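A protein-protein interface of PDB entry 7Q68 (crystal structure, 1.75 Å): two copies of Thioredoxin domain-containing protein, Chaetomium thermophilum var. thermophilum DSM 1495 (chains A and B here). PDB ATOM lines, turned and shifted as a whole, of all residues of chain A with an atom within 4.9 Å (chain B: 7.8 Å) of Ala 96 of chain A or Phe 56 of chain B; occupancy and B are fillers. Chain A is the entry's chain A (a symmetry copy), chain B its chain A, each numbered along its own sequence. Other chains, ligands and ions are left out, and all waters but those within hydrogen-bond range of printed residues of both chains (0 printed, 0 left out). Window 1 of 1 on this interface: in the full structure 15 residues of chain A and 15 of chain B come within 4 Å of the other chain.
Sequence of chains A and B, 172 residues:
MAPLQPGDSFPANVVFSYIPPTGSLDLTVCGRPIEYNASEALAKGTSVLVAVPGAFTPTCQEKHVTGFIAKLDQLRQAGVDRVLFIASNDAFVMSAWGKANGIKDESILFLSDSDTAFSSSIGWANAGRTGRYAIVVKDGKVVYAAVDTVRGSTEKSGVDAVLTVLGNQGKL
Of the printed residues of chain B, Val 93 of chain A touches Asn 89 and Val 93.
Ser 95 of chain A touches none of the printed residues of chain B.
Of chain A, only Leu 27 (3.8 Å), Phe 92 (3.4 Å) and Ala 96 (3.5 Å) come within 4 Å of Phe 56 of chain B.
Gln 61 of chain B touches none of the printed residues of chain A.
Of the printed residues of chain A, Phe 92 of chain B touches Phe 56.
The nearest residue of chain B that does not touch Ala 96 of chain A is Leu 27 of chain B (5.5 Å).
The nearest printed residue of chain B that does not touch Ala 100 of chain A is Ala 96 of chain B (6.7 Å).
Leu 27 of chain A touches its own counterpart, Leu 27 of chain B.
Leu 27 of chain A touches Phe 56 of chain B, and with the chains exchanged Phe 56 of chain A touches Leu 27 of chain B.
Phe 56 of chain A touches Phe 92 of chain B, and with the chains exchanged Phe 92 of chain A touches Phe 56 of chain B.
Val 93 of chain B touches its own counterpart, Val 93 of chain A.
Of the 12 pairs that touch across the chains among the printed residues, 10 have their exchanged pair printed and touching as well.
Of the 11 printed residues of chain A, 6 touch a printed residue of chain B.
Along chain B the printed residues that touch a printed residue of chain A span positions 27 to 100.
Among the printed residues, no Asp or Glu carboxylate lies within 4 Å of a Lys or Arg side-chain nitrogen of the other chain.
CD2 of Leu 27 of chain A touches CD2 of Leu 27 of chain B, 3.7 Å away.
CD2 of Leu 27 of chain A touches CE1 of Phe 56 of chain B, at 3.8 Å.
CB of Ala 100 of chain B touches CD2 of Leu 27 of chain A, 3.96 Å away.
CE1 of Phe 56 of chain A touches CD2 of Leu 27 of chain B (3.8 Å).
Ala 96 of chain B touches Phe 56 of chain A.
CB of Phe 92 of chain A touches O of Phe 56 of chain B (3.4 Å).
Phe 92 of chain A touches Pro 58 of chain B (CE1 to CD, 3.5 Å).
CG2 of Val 93 of chain A touches ND2 of Asn 89 of chain B, 3.8 Å away.
Val 93 of chain B touches Val 93 of chain A (CG1 to CG2, 3.9 Å).
Ala 100 of chain A touches Leu 27 of chain B (CB to CD2, 3.96 Å).
The side-chain amide oxygen (OD1) of Asn 89 of chain B sits at hydrogen-bond distance from the backbone NH (N) of Ala 55 of chain B, 2.9 Å away.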
ATOM      1  N   LEU A  27      24.645  -7.631  15.325  1.00  0.00           N
ATOM      2  CA  LEU A  27      25.304  -8.034  14.089  1.00  0.00           C
ATOM      3  C   LEU A  27      24.603  -7.529  12.835  1.00  0.00           C
ATOM      4  O   LEU A  27      25.111  -7.769  11.733  1.00  0.00           O
ATOM      5  CB  LEU A  27      25.421  -9.558  14.037  1.00  0.00           C
ATOM      6  CG  LEU A  27      26.656 -10.128  14.733  1.00  0.00           C
ATOM      7  CD1 LEU A  27      26.595  -9.905  16.241  1.00  0.00           C
ATOM      8  CD2 LEU A  27      26.815 -11.609  14.428  1.00  0.00           C
ATOM      9  N   PHE A  56      35.594 -17.000  13.196  1.00  0.00           N
ATOM     10  CA  PHE A  56      34.488 -17.904  13.487  1.00  0.00           C
ATOM     11  C   PHE A  56      34.894 -19.375  13.481  1.00  0.00           C
ATOM     12  O   PHE A  56      34.046 -20.251  13.287  1.00  0.00           O
ATOM     13  CB  PHE A  56      33.326 -17.688  12.509  1.00  0.00           C
ATOM     14  CG  PHE A  56      32.554 -16.415  12.748  1.00  0.00           C
ATOM     15  CD1 PHE A  56      31.690 -16.309  13.820  1.00  0.00           C
ATOM     16  CD2 PHE A  56      32.710 -15.326  11.902  1.00  0.00           C
ATOM     17  CE1 PHE A  56      30.981 -15.142  14.048  1.00  0.00           C
ATOM     18  CE2 PHE A  56      31.997 -14.151  12.130  1.00  0.00           C
ATOM     19  CZ  PHE A  56      31.143 -14.065  13.180  1.00  0.00           C
ATOM     20  N   PHE A  92      33.742  -6.886   7.023  1.00  0.00           N
ATOM     21  CA  PHE A  92      32.399  -7.164   7.516  1.00  0.00           C
ATOM     22  C   PHE A  92      32.381  -8.411   8.390  1.00  0.00           C
ATOM     23  O   PHE A  92      31.738  -8.439   9.447  1.00  0.00           O
ATOM     24  CB  PHE A  92      31.441  -7.337   6.345  1.00  0.00           C
ATOM     25  CG  PHE A  92      31.312  -6.110   5.497  1.00  0.00           C
ATOM     26  CD1 PHE A  92      30.448  -5.101   5.865  1.00  0.00           C
ATOM     27  CD2 PHE A  92      32.069  -5.968   4.347  1.00  0.00           C
ATOM     28  CE1 PHE A  92      30.345  -3.950   5.095  1.00  0.00           C
ATOM     29  CE2 PHE A  92      31.951  -4.813   3.565  1.00  0.00           C
ATOM     30  CZ  PHE A  92      31.094  -3.832   3.950  1.00  0.00           C
ATOM     31  N   VAL A  93      33.076  -9.460   7.959  1.00  0.00           N
ATOM     32  CA  VAL A  93      33.124 -10.694   8.741  1.00  0.00           C
ATOM     33  C   VAL A  93      33.888 -10.475  10.039  1.00  0.00           C
ATOM     34  O   VAL A  93      33.475 -10.946  11.107  1.00  0.00           O
ATOM     35  CB  VAL A  93      33.752 -11.824   7.903  1.00  0.00           C
ATOM     36  CG1 VAL A  93      33.947 -13.087   8.743  1.00  0.00           C
ATOM     37  CG2 VAL A  93      32.901 -12.119   6.681  1.00  0.00           C
ATOM     38  N   MET A  94      35.012  -9.762   9.972  1.00  0.00           N
ATOM     39  CA  MET A  94      35.791  -9.499  11.179  1.00  0.00           C
ATOM     40  C   MET A  94      34.999  -8.674  12.187  1.00  0.00           C
ATOM     41  O   MET A  94      35.066  -8.923  13.399  1.00  0.00           O
ATOM     42  CB  MET A  94      37.093  -8.791  10.824  1.00  0.00           C
ATOM     43  CG  MET A  94      38.055  -9.625   9.987  1.00  0.00           C
ATOM     44  SD  MET A  94      38.569 -11.127  10.803  1.00  0.00           S
ATOM     45  CE  MET A  94      39.572 -10.483  12.141  1.00  0.00           C
ATOM     46  N   SER A  95      34.234  -7.691  11.710  1.00  0.00           N
ATOM     47  CA  SER A  95      33.400  -6.907  12.615  1.00  0.00           C
ATOM     48  C   SER A  95      32.377  -7.783  13.329  1.00  0.00           C
ATOM     49  O   SER A  95      32.180  -7.667  14.548  1.00  0.00           O
ATOM     50  CB  SER A  95      32.701  -5.786  11.829  1.00  0.00           C
ATOM     51  OG  SER A  95      31.796  -5.099  12.669  1.00  0.00           O
ATOM     52  N   ALA A  96      31.698  -8.656  12.580  1.00  0.00           N
ATOM     53  CA  ALA A  96      30.723  -9.546  13.199  1.00  0.00           C
ATOM     54  C   ALA A  96      31.396 -10.479  14.194  1.00  0.00           C
ATOM     55  O   ALA A  96      30.821 -10.808  15.239  1.00  0.00           O
ATOM     56  CB  ALA A  96      29.987 -10.357  12.134  1.00  0.00           C
ATOM     57  N   TRP A  97      32.606 -10.931  13.878  1.00  0.00           N
ATOM     58  CA  TRP A  97      33.311 -11.848  14.775  1.00  0.00           C
ATOM     59  C   TRP A  97      33.682 -11.142  16.076  1.00  0.00           C
ATOM     60  O   TRP A  97      33.566 -11.720  17.165  1.00  0.00           O
ATOM     61  CB  TRP A  97      34.550 -12.403  14.072  1.00  0.00           C
ATOM     62  CG  TRP A  97      35.261 -13.502  14.849  1.00  0.00           C
ATOM     63  CD1 TRP A  97      34.694 -14.583  15.440  1.00  0.00           C
ATOM     64  CD2 TRP A  97      36.669 -13.600  15.086  1.00  0.00           C
ATOM     65  NE1 TRP A  97      35.666 -15.354  16.056  1.00  0.00           N
ATOM     66  CE2 TRP A  97      36.887 -14.767  15.845  1.00  0.00           C
ATOM     67  CE3 TRP A  97      37.769 -12.808  14.732  1.00  0.00           C
ATOM     68  CZ2 TRP A  97      38.157 -15.166  16.257  1.00  0.00           C
ATOM     69  CZ3 TRP A  97      39.030 -13.196  15.147  1.00  0.00           C
ATOM     70  CH2 TRP A  97      39.215 -14.373  15.904  1.00  0.00           C
ATOM     71  N   GLY A  98      34.118  -9.888  15.981  1.00  0.00           N
ATOM     72  CA  GLY A  98      34.382  -9.114  17.184  1.00  0.00           C
ATOM     73  C   GLY A  98      33.151  -8.969  18.052  1.00  0.00           C
ATOM     74  O   GLY A  98      33.204  -9.158  19.271  1.00  0.00           O
ATOM     75  N   LYS A  99      32.020  -8.630  17.429  1.00  0.00           N
ATOM     76  CA  LYS A  99      30.782  -8.492  18.182  1.00  0.00           C
ATOM     77  C   LYS A  99      30.327  -9.830  18.750  1.00  0.00           C
ATOM     78  O   LYS A  99      29.779  -9.883  19.855  1.00  0.00           O
ATOM     79  CB  LYS A  99      29.691  -7.913  17.295  1.00  0.00           C
ATOM     80  CG  LYS A  99      29.928  -6.466  16.878  1.00  0.00           C
ATOM     81  CD  LYS A  99      28.841  -6.050  15.906  1.00  0.00           C
ATOM     82  CE  LYS A  99      29.099  -4.676  15.315  1.00  0.00           C
ATOM     83  NZ  LYS A  99      28.022  -4.360  14.327  1.00  0.00           N
ATOM     84  N   ALA A 100      30.509 -10.914  17.994  1.00  0.00           N
ATOM     85  CA  ALA A 100      30.133 -12.229  18.502  1.00  0.00           C
ATOM     86  C   ALA A 100      30.915 -12.567  19.761  1.00  0.00           C
ATOM     87  O   ALA A 100      30.434 -13.327  20.612  1.00  0.00           O
ATOM     88  CB  ALA A 100      30.372 -13.304  17.435  1.00  0.00           C
ATOM     89  N   LEU B  27      26.490 -18.476  18.466  1.00  0.00           N
ATOM     90  CA  LEU B  27      27.587 -18.411  17.509  1.00  0.00           C
ATOM     91  C   LEU B  27      28.880 -19.028  18.024  1.00  0.00           C
ATOM     92  O   LEU B  27      29.859 -19.073  17.269  1.00  0.00           O
ATOM     93  CB  LEU B  27      27.835 -16.956  17.105  1.00  0.00           C
ATOM     94  CG  LEU B  27      26.966 -16.457  15.952  1.00  0.00           C
ATOM     95  CD1 LEU B  27      25.497 -16.387  16.355  1.00  0.00           C
ATOM     96  CD2 LEU B  27      27.442 -15.097  15.466  1.00  0.00           C
ATOM     97  N   VAL B  52      24.965 -14.944  -2.830  1.00  0.00           N
ATOM     98  CA  VAL B  52      25.203 -13.546  -2.470  1.00  0.00           C
ATOM     99  C   VAL B  52      26.697 -13.259  -2.557  1.00  0.00           C
ATOM    100  O   VAL B  52      27.519 -14.161  -2.332  1.00  0.00           O
ATOM    101  CB  VAL B  52      24.660 -13.225  -1.063  1.00  0.00           C
ATOM    102  CG1 VAL B  52      23.157 -13.481  -0.999  1.00  0.00           C
ATOM    103  CG2 VAL B  52      25.398 -14.018   0.018  1.00  0.00           C
ATOM    104  N   PRO B  53      27.097 -12.024  -2.860  1.00  0.00           N
ATOM    105  CA  PRO B  53      28.537 -11.736  -2.959  1.00  0.00           C
ATOM    106  C   PRO B  53      29.275 -11.932  -1.651  1.00  0.00           C
ATOM    107  O   PRO B  53      30.480 -12.223  -1.660  1.00  0.00           O
ATOM    108  CB  PRO B  53      28.568 -10.272  -3.405  1.00  0.00           C
ATOM    109  CG  PRO B  53      27.262 -10.052  -4.109  1.00  0.00           C
ATOM    110  CD  PRO B  53      26.264 -10.906  -3.352  1.00  0.00           C
ATOM    111  N   GLY B  54      28.601 -11.783  -0.517  1.00  0.00           N
ATOM    112  CA  GLY B  54      29.295 -11.963   0.744  1.00  0.00           C
ATOM    113  C   GLY B  54      28.421 -12.063   1.971  1.00  0.00           C
ATOM    114  O   GLY B  54      27.454 -11.324   2.136  1.00  0.00           O
ATOM    115  N   ALA B  55      28.758 -13.001   2.862  1.00  0.00           N
ATOM    116  CA  ALA B  55      28.101 -13.036   4.156  1.00  0.00           C
ATOM    117  C   ALA B  55      28.369 -11.749   4.926  1.00  0.00           C
ATOM    118  O   ALA B  55      29.419 -11.121   4.780  1.00  0.00           O
ATOM    119  CB  ALA B  55      28.603 -14.241   4.967  1.00  0.00           C
ATOM    120  N   PHE B  56      27.407 -11.381   5.778  1.00  0.00           N
ATOM    121  CA  PHE B  56      27.515 -10.285   6.734  1.00  0.00           C
ATOM    122  C   PHE B  56      27.644  -8.917   6.071  1.00  0.00           C
ATOM    123  O   PHE B  56      28.155  -7.977   6.687  1.00  0.00           O
ATOM    124  CB  PHE B  56      28.691 -10.504   7.695  1.00  0.00           C
ATOM    125  CG  PHE B  56      28.450 -11.584   8.721  1.00  0.00           C
ATOM    126  CD1 PHE B  56      27.601 -11.362   9.787  1.00  0.00           C
ATOM    127  CD2 PHE B  56      29.067 -12.820   8.600  1.00  0.00           C
ATOM    128  CE1 PHE B  56      27.373 -12.348  10.730  1.00  0.00           C
ATOM    129  CE2 PHE B  56      28.838 -13.814   9.549  1.00  0.00           C
ATOM    130  CZ  PHE B  56      28.011 -13.578  10.597  1.00  0.00           C
ATOM    131  N   THR B  57      27.204  -8.772   4.849  1.00  0.00           N
ATOM    132  CA  THR B  57      27.163  -7.400   4.325  1.00  0.00           C
ATOM    133  C   THR B  57      25.945  -6.660   4.884  1.00  0.00           C
ATOM    134  O   THR B  57      24.897  -7.263   5.122  1.00  0.00           O
ATOM    135  CB  THR B  57      27.127  -7.394   2.804  1.00  0.00           C
ATOM    136  OG1 THR B  57      25.947  -8.060   2.350  1.00  0.00           O
ATOM    137  CG2 THR B  57      28.363  -8.091   2.251  1.00  0.00           C
ATOM    138  N   PRO B  58      26.056  -5.349   5.088  1.00  0.00           N
ATOM    139  CA  PRO B  58      25.101  -4.663   5.969  1.00  0.00           C
ATOM    140  C   PRO B  58      23.709  -4.589   5.366  1.00  0.00           C
ATOM    141  O   PRO B  58      23.529  -4.615   4.146  1.00  0.00           O
ATOM    142  CB  PRO B  58      25.713  -3.264   6.134  1.00  0.00           C
ATOM    143  CG  PRO B  58      26.449  -3.037   4.838  1.00  0.00           C
ATOM    144  CD  PRO B  58      26.931  -4.405   4.359  1.00  0.00           C
ATOM    145  N   THR B  59      22.710  -4.499   6.251  1.00  0.00           N
ATOM    146  CA  THR B  59      21.333  -4.364   5.787  1.00  0.00           C
ATOM    147  C   THR B  59      21.129  -3.059   5.035  1.00  0.00           C
ATOM    148  O   THR B  59      20.352  -3.020   4.076  1.00  0.00           O
ATOM    149  CB  THR B  59      20.358  -4.434   6.969  1.00  0.00           C
ATOM    150  OG1 THR B  59      20.648  -3.385   7.903  1.00  0.00           O
ATOM    151  CG2 THR B  59      20.459  -5.787   7.672  1.00  0.00           C
ATOM    152  N   GLN B  61      22.661  -1.820   2.814  1.00  0.00           N
ATOM    153  CA  GLN B  61      22.781  -2.125   1.398  1.00  0.00           C
ATOM    154  C   GLN B  61      22.035  -3.390   0.994  1.00  0.00           C
ATOM    155  O   GLN B  61      21.714  -3.546  -0.190  1.00  0.00           O
ATOM    156  CB  GLN B  61      24.255  -2.302   1.010  1.00  0.00           C
ATOM    157  CG  GLN B  61      25.194  -1.225   1.509  1.00  0.00           C
ATOM    158  CD  GLN B  61      26.648  -1.537   1.188  1.00  0.00           C
ATOM    159  OE1 GLN B  61      27.231  -2.486   1.724  1.00  0.00           O
ATOM    160  NE2 GLN B  61      27.237  -0.745   0.297  1.00  0.00           N
ATOM    161  N   GLU B  62      21.746  -4.288   1.939  1.00  0.00           N
ATOM    162  CA  GLU B  62      21.356  -5.656   1.614  1.00  0.00           C
ATOM    163  C   GLU B  62      20.159  -6.097   2.441  1.00  0.00           C
ATOM    164  O   GLU B  62      20.244  -6.194   3.669  1.00  0.00           O
ATOM    165  CB  GLU B  62      22.535  -6.612   1.851  1.00  0.00           C
ATOM    166  CG  GLU B  62      22.767  -7.605   0.741  1.00  0.00           C
ATOM    167  CD  GLU B  62      23.294  -8.936   1.245  1.00  0.00           C
ATOM    168  OE1 GLU B  62      23.892  -8.974   2.342  1.00  0.00           O
ATOM    169  OE2 GLU B  62      23.091  -9.948   0.548  1.00  0.00           O
ATOM    170  N   ALA B  87      27.645 -18.548  -0.673  1.00  0.00           N
ATOM    171  CA  ALA B  87      28.600 -17.472  -0.920  1.00  0.00           C
ATOM    172  C   ALA B  87      29.982 -18.111  -0.910  1.00  0.00           C
ATOM    173  O   ALA B  87      30.127 -19.305  -0.631  1.00  0.00           O
ATOM    174  CB  ALA B  87      28.474 -16.366   0.117  1.00  0.00           C
ATOM    175  N   ASN B  89      32.342 -17.292   1.181  1.00  0.00           N
ATOM    176  CA  ASN B  89      32.808 -17.441   2.558  1.00  0.00           C
ATOM    177  C   ASN B  89      32.811 -18.908   2.959  1.00  0.00           C
ATOM    178  O   ASN B  89      31.993 -19.692   2.490  1.00  0.00           O
ATOM    179  CB  ASN B  89      31.920 -16.657   3.521  1.00  0.00           C
ATOM    180  CG  ASN B  89      31.687 -15.225   3.056  1.00  0.00           C
ATOM    181  OD1 ASN B  89      30.820 -14.979   2.220  1.00  0.00           O
ATOM    182  ND2 ASN B  89      32.463 -14.289   3.583  1.00  0.00           N
ATOM    183  N   PHE B  92      32.279 -22.073   8.181  1.00  0.00           N
ATOM    184  CA  PHE B  92      32.154 -21.514   9.520  1.00  0.00           C
ATOM    185  C   PHE B  92      31.501 -20.138   9.484  1.00  0.00           C
ATOM    186  O   PHE B  92      30.636 -19.821  10.310  1.00  0.00           O
ATOM    187  CB  PHE B  92      33.526 -21.420  10.175  1.00  0.00           C
ATOM    188  CG  PHE B  92      34.190 -22.749  10.353  1.00  0.00           C
ATOM    189  CD1 PHE B  92      33.885 -23.534  11.445  1.00  0.00           C
ATOM    190  CD2 PHE B  92      35.102 -23.210   9.421  1.00  0.00           C
ATOM    191  CE1 PHE B  92      34.480 -24.780  11.601  1.00  0.00           C
ATOM    192  CE2 PHE B  92      35.711 -24.460   9.589  1.00  0.00           C
ATOM    193  CZ  PHE B  92      35.392 -25.216  10.672  1.00  0.00           C
ATOM    194  N   VAL B  93      31.910 -19.301   8.535  1.00  0.00           N
ATOM    195  CA  VAL B  93      31.329 -17.965   8.419  1.00  0.00           C
ATOM    196  C   VAL B  93      29.873 -18.051   7.986  1.00  0.00           C
ATOM    197  O   VAL B  93      29.010 -17.335   8.512  1.00  0.00           O
ATOM    198  CB  VAL B  93      32.158 -17.114   7.438  1.00  0.00           C
ATOM    199  CG1 VAL B  93      31.492 -15.760   7.187  1.00  0.00           C
ATOM    200  CG2 VAL B  93      33.573 -16.927   7.956  1.00  0.00           C
ATOM    201  N   MET B  94      29.575 -18.922   7.023  1.00  0.00           N
ATOM    202  CA  MET B  94      28.196 -19.071   6.565  1.00  0.00           C
ATOM    203  C   MET B  94      27.287 -19.570   7.682  1.00  0.00           C
ATOM    204  O   MET B  94      26.141 -19.114   7.815  1.00  0.00           O
ATOM    205  CB  MET B  94      28.135 -20.016   5.371  1.00  0.00           C
ATOM    206  CG  MET B  94      28.842 -19.502   4.123  1.00  0.00           C
ATOM    207  SD  MET B  94      28.160 -17.967   3.516  1.00  0.00           S
ATOM    208  CE  MET B  94      26.547 -18.495   2.939  1.00  0.00           C
ATOM    209  N   SER B  95      27.775 -20.499   8.502  1.00  0.00           N
ATOM    210  CA  SER B  95      26.981 -20.972   9.631  1.00  0.00           C
ATOM    211  C   SER B  95      26.658 -19.838  10.598  1.00  0.00           C
ATOM    212  O   SER B  95      25.513 -19.697  11.054  1.00  0.00           O
ATOM    213  CB  SER B  95      27.732 -22.102  10.352  1.00  0.00           C
ATOM    214  OG  SER B  95      27.030 -22.482  11.518  1.00  0.00           O
ATOM    215  N   ALA B  96      27.663 -19.027  10.940  1.00  0.00           N
ATOM    216  CA  ALA B  96      27.423 -17.905  11.838  1.00  0.00           C
ATOM    217  C   ALA B  96      26.449 -16.914  11.219  1.00  0.00           C
ATOM    218  O   ALA B  96      25.624 -16.317  11.921  1.00  0.00           O
ATOM    219  CB  ALA B  96      28.736 -17.204  12.182  1.00  0.00           C
ATOM    220  N   TRP B  97      26.541 -16.711   9.908  1.00  0.00           N
ATOM    221  CA  TRP B  97      25.652 -15.760   9.242  1.00  0.00           C
ATOM    222  C   TRP B  97      24.211 -16.260   9.276  1.00  0.00           C
ATOM    223  O   TRP B  97      23.275 -15.481   9.500  1.00  0.00           O
ATOM    224  CB  TRP B  97      26.126 -15.533   7.806  1.00  0.00           C
ATOM    225  CG  TRP B  97      25.377 -14.426   7.076  1.00  0.00           C
ATOM    226  CD1 TRP B  97      25.098 -13.183   7.541  1.00  0.00           C
ATOM    227  CD2 TRP B  97      24.840 -14.495   5.750  1.00  0.00           C
ATOM    228  NE1 TRP B  97      24.396 -12.463   6.587  1.00  0.00           N
ATOM    229  CE2 TRP B  97      24.232 -13.253   5.479  1.00  0.00           C
ATOM    230  CE3 TRP B  97      24.811 -15.492   4.767  1.00  0.00           C
ATOM    231  CZ2 TRP B  97      23.604 -12.978   4.267  1.00  0.00           C
ATOM    232  CZ3 TRP B  97      24.180 -15.225   3.566  1.00  0.00           C
ATOM    233  CH2 TRP B  97      23.583 -13.968   3.324  1.00  0.00           C
ATOM    234  N   GLY B  98      24.018 -17.561   9.069  1.00  0.00           N
ATOM    235  CA  GLY B  98      22.685 -18.130   9.200  1.00  0.00           C
ATOM    236  C   GLY B  98      22.112 -17.930  10.586  1.00  0.00           C
ATOM    237  O   GLY B  98      20.955 -17.530  10.745  1.00  0.00           O
ATOM    238  N   LYS B  99      22.920 -18.206  11.611  1.00  0.00           N
ATOM    239  CA  LYS B  99      22.459 -18.019  12.979  1.00  0.00           C
ATOM    240  C   LYS B  99      22.215 -16.548  13.285  1.00  0.00           C
ATOM    241  O   LYS B  99      21.286 -16.211  14.024  1.00  0.00           O
ATOM    242  CB  LYS B  99      23.478 -18.585  13.957  1.00  0.00           C
ATOM    243  CG  LYS B  99      23.612 -20.102  13.911  1.00  0.00           C
ATOM    244  CD  LYS B  99      24.734 -20.526  14.838  1.00  0.00           C
ATOM    245  CE  LYS B  99      25.042 -22.008  14.724  1.00  0.00           C
ATOM    246  NZ  LYS B  99      26.193 -22.338  15.620  1.00  0.00           N
ATOM    247  N   ALA B 100      23.061 -15.660  12.757  1.00  0.00           N
ATOM    248  CA  ALA B 100      22.852 -14.233  12.979  1.00  0.00           C
ATOM    249  C   ALA B 100      21.511 -13.789  12.418  1.00  0.00           C
ATOM    250  O   ALA B 100      20.916 -12.822  12.912  1.00  0.00           O
ATOM    251  CB  ALA B 100      23.982 -13.420  12.336  1.00  0.00           C
ATOM    252  N   ASN B 101      21.029 -14.474  11.383  1.00  0.00           N
ATOM    253  CA  ASN B 101      19.740 -14.177  10.774  1.00  0.00           C
ATOM    254  C   ASN B 101      18.596 -14.981  11.382  1.00  0.00           C
ATOM    255  O   ASN B 101      17.488 -14.963  10.839  1.00  0.00           O
ATOM    256  CB  ASN B 101      19.814 -14.431   9.271  1.00  0.00           C
ATOM    257  CG  ASN B 101      20.488 -13.293   8.527  1.00  0.00           C
ATOM    258  OD1 ASN B 101      19.871 -12.267   8.252  1.00  0.00           O
ATOM    259  ND2 ASN B 101      21.764 -13.469   8.213  1.00  0.00           N
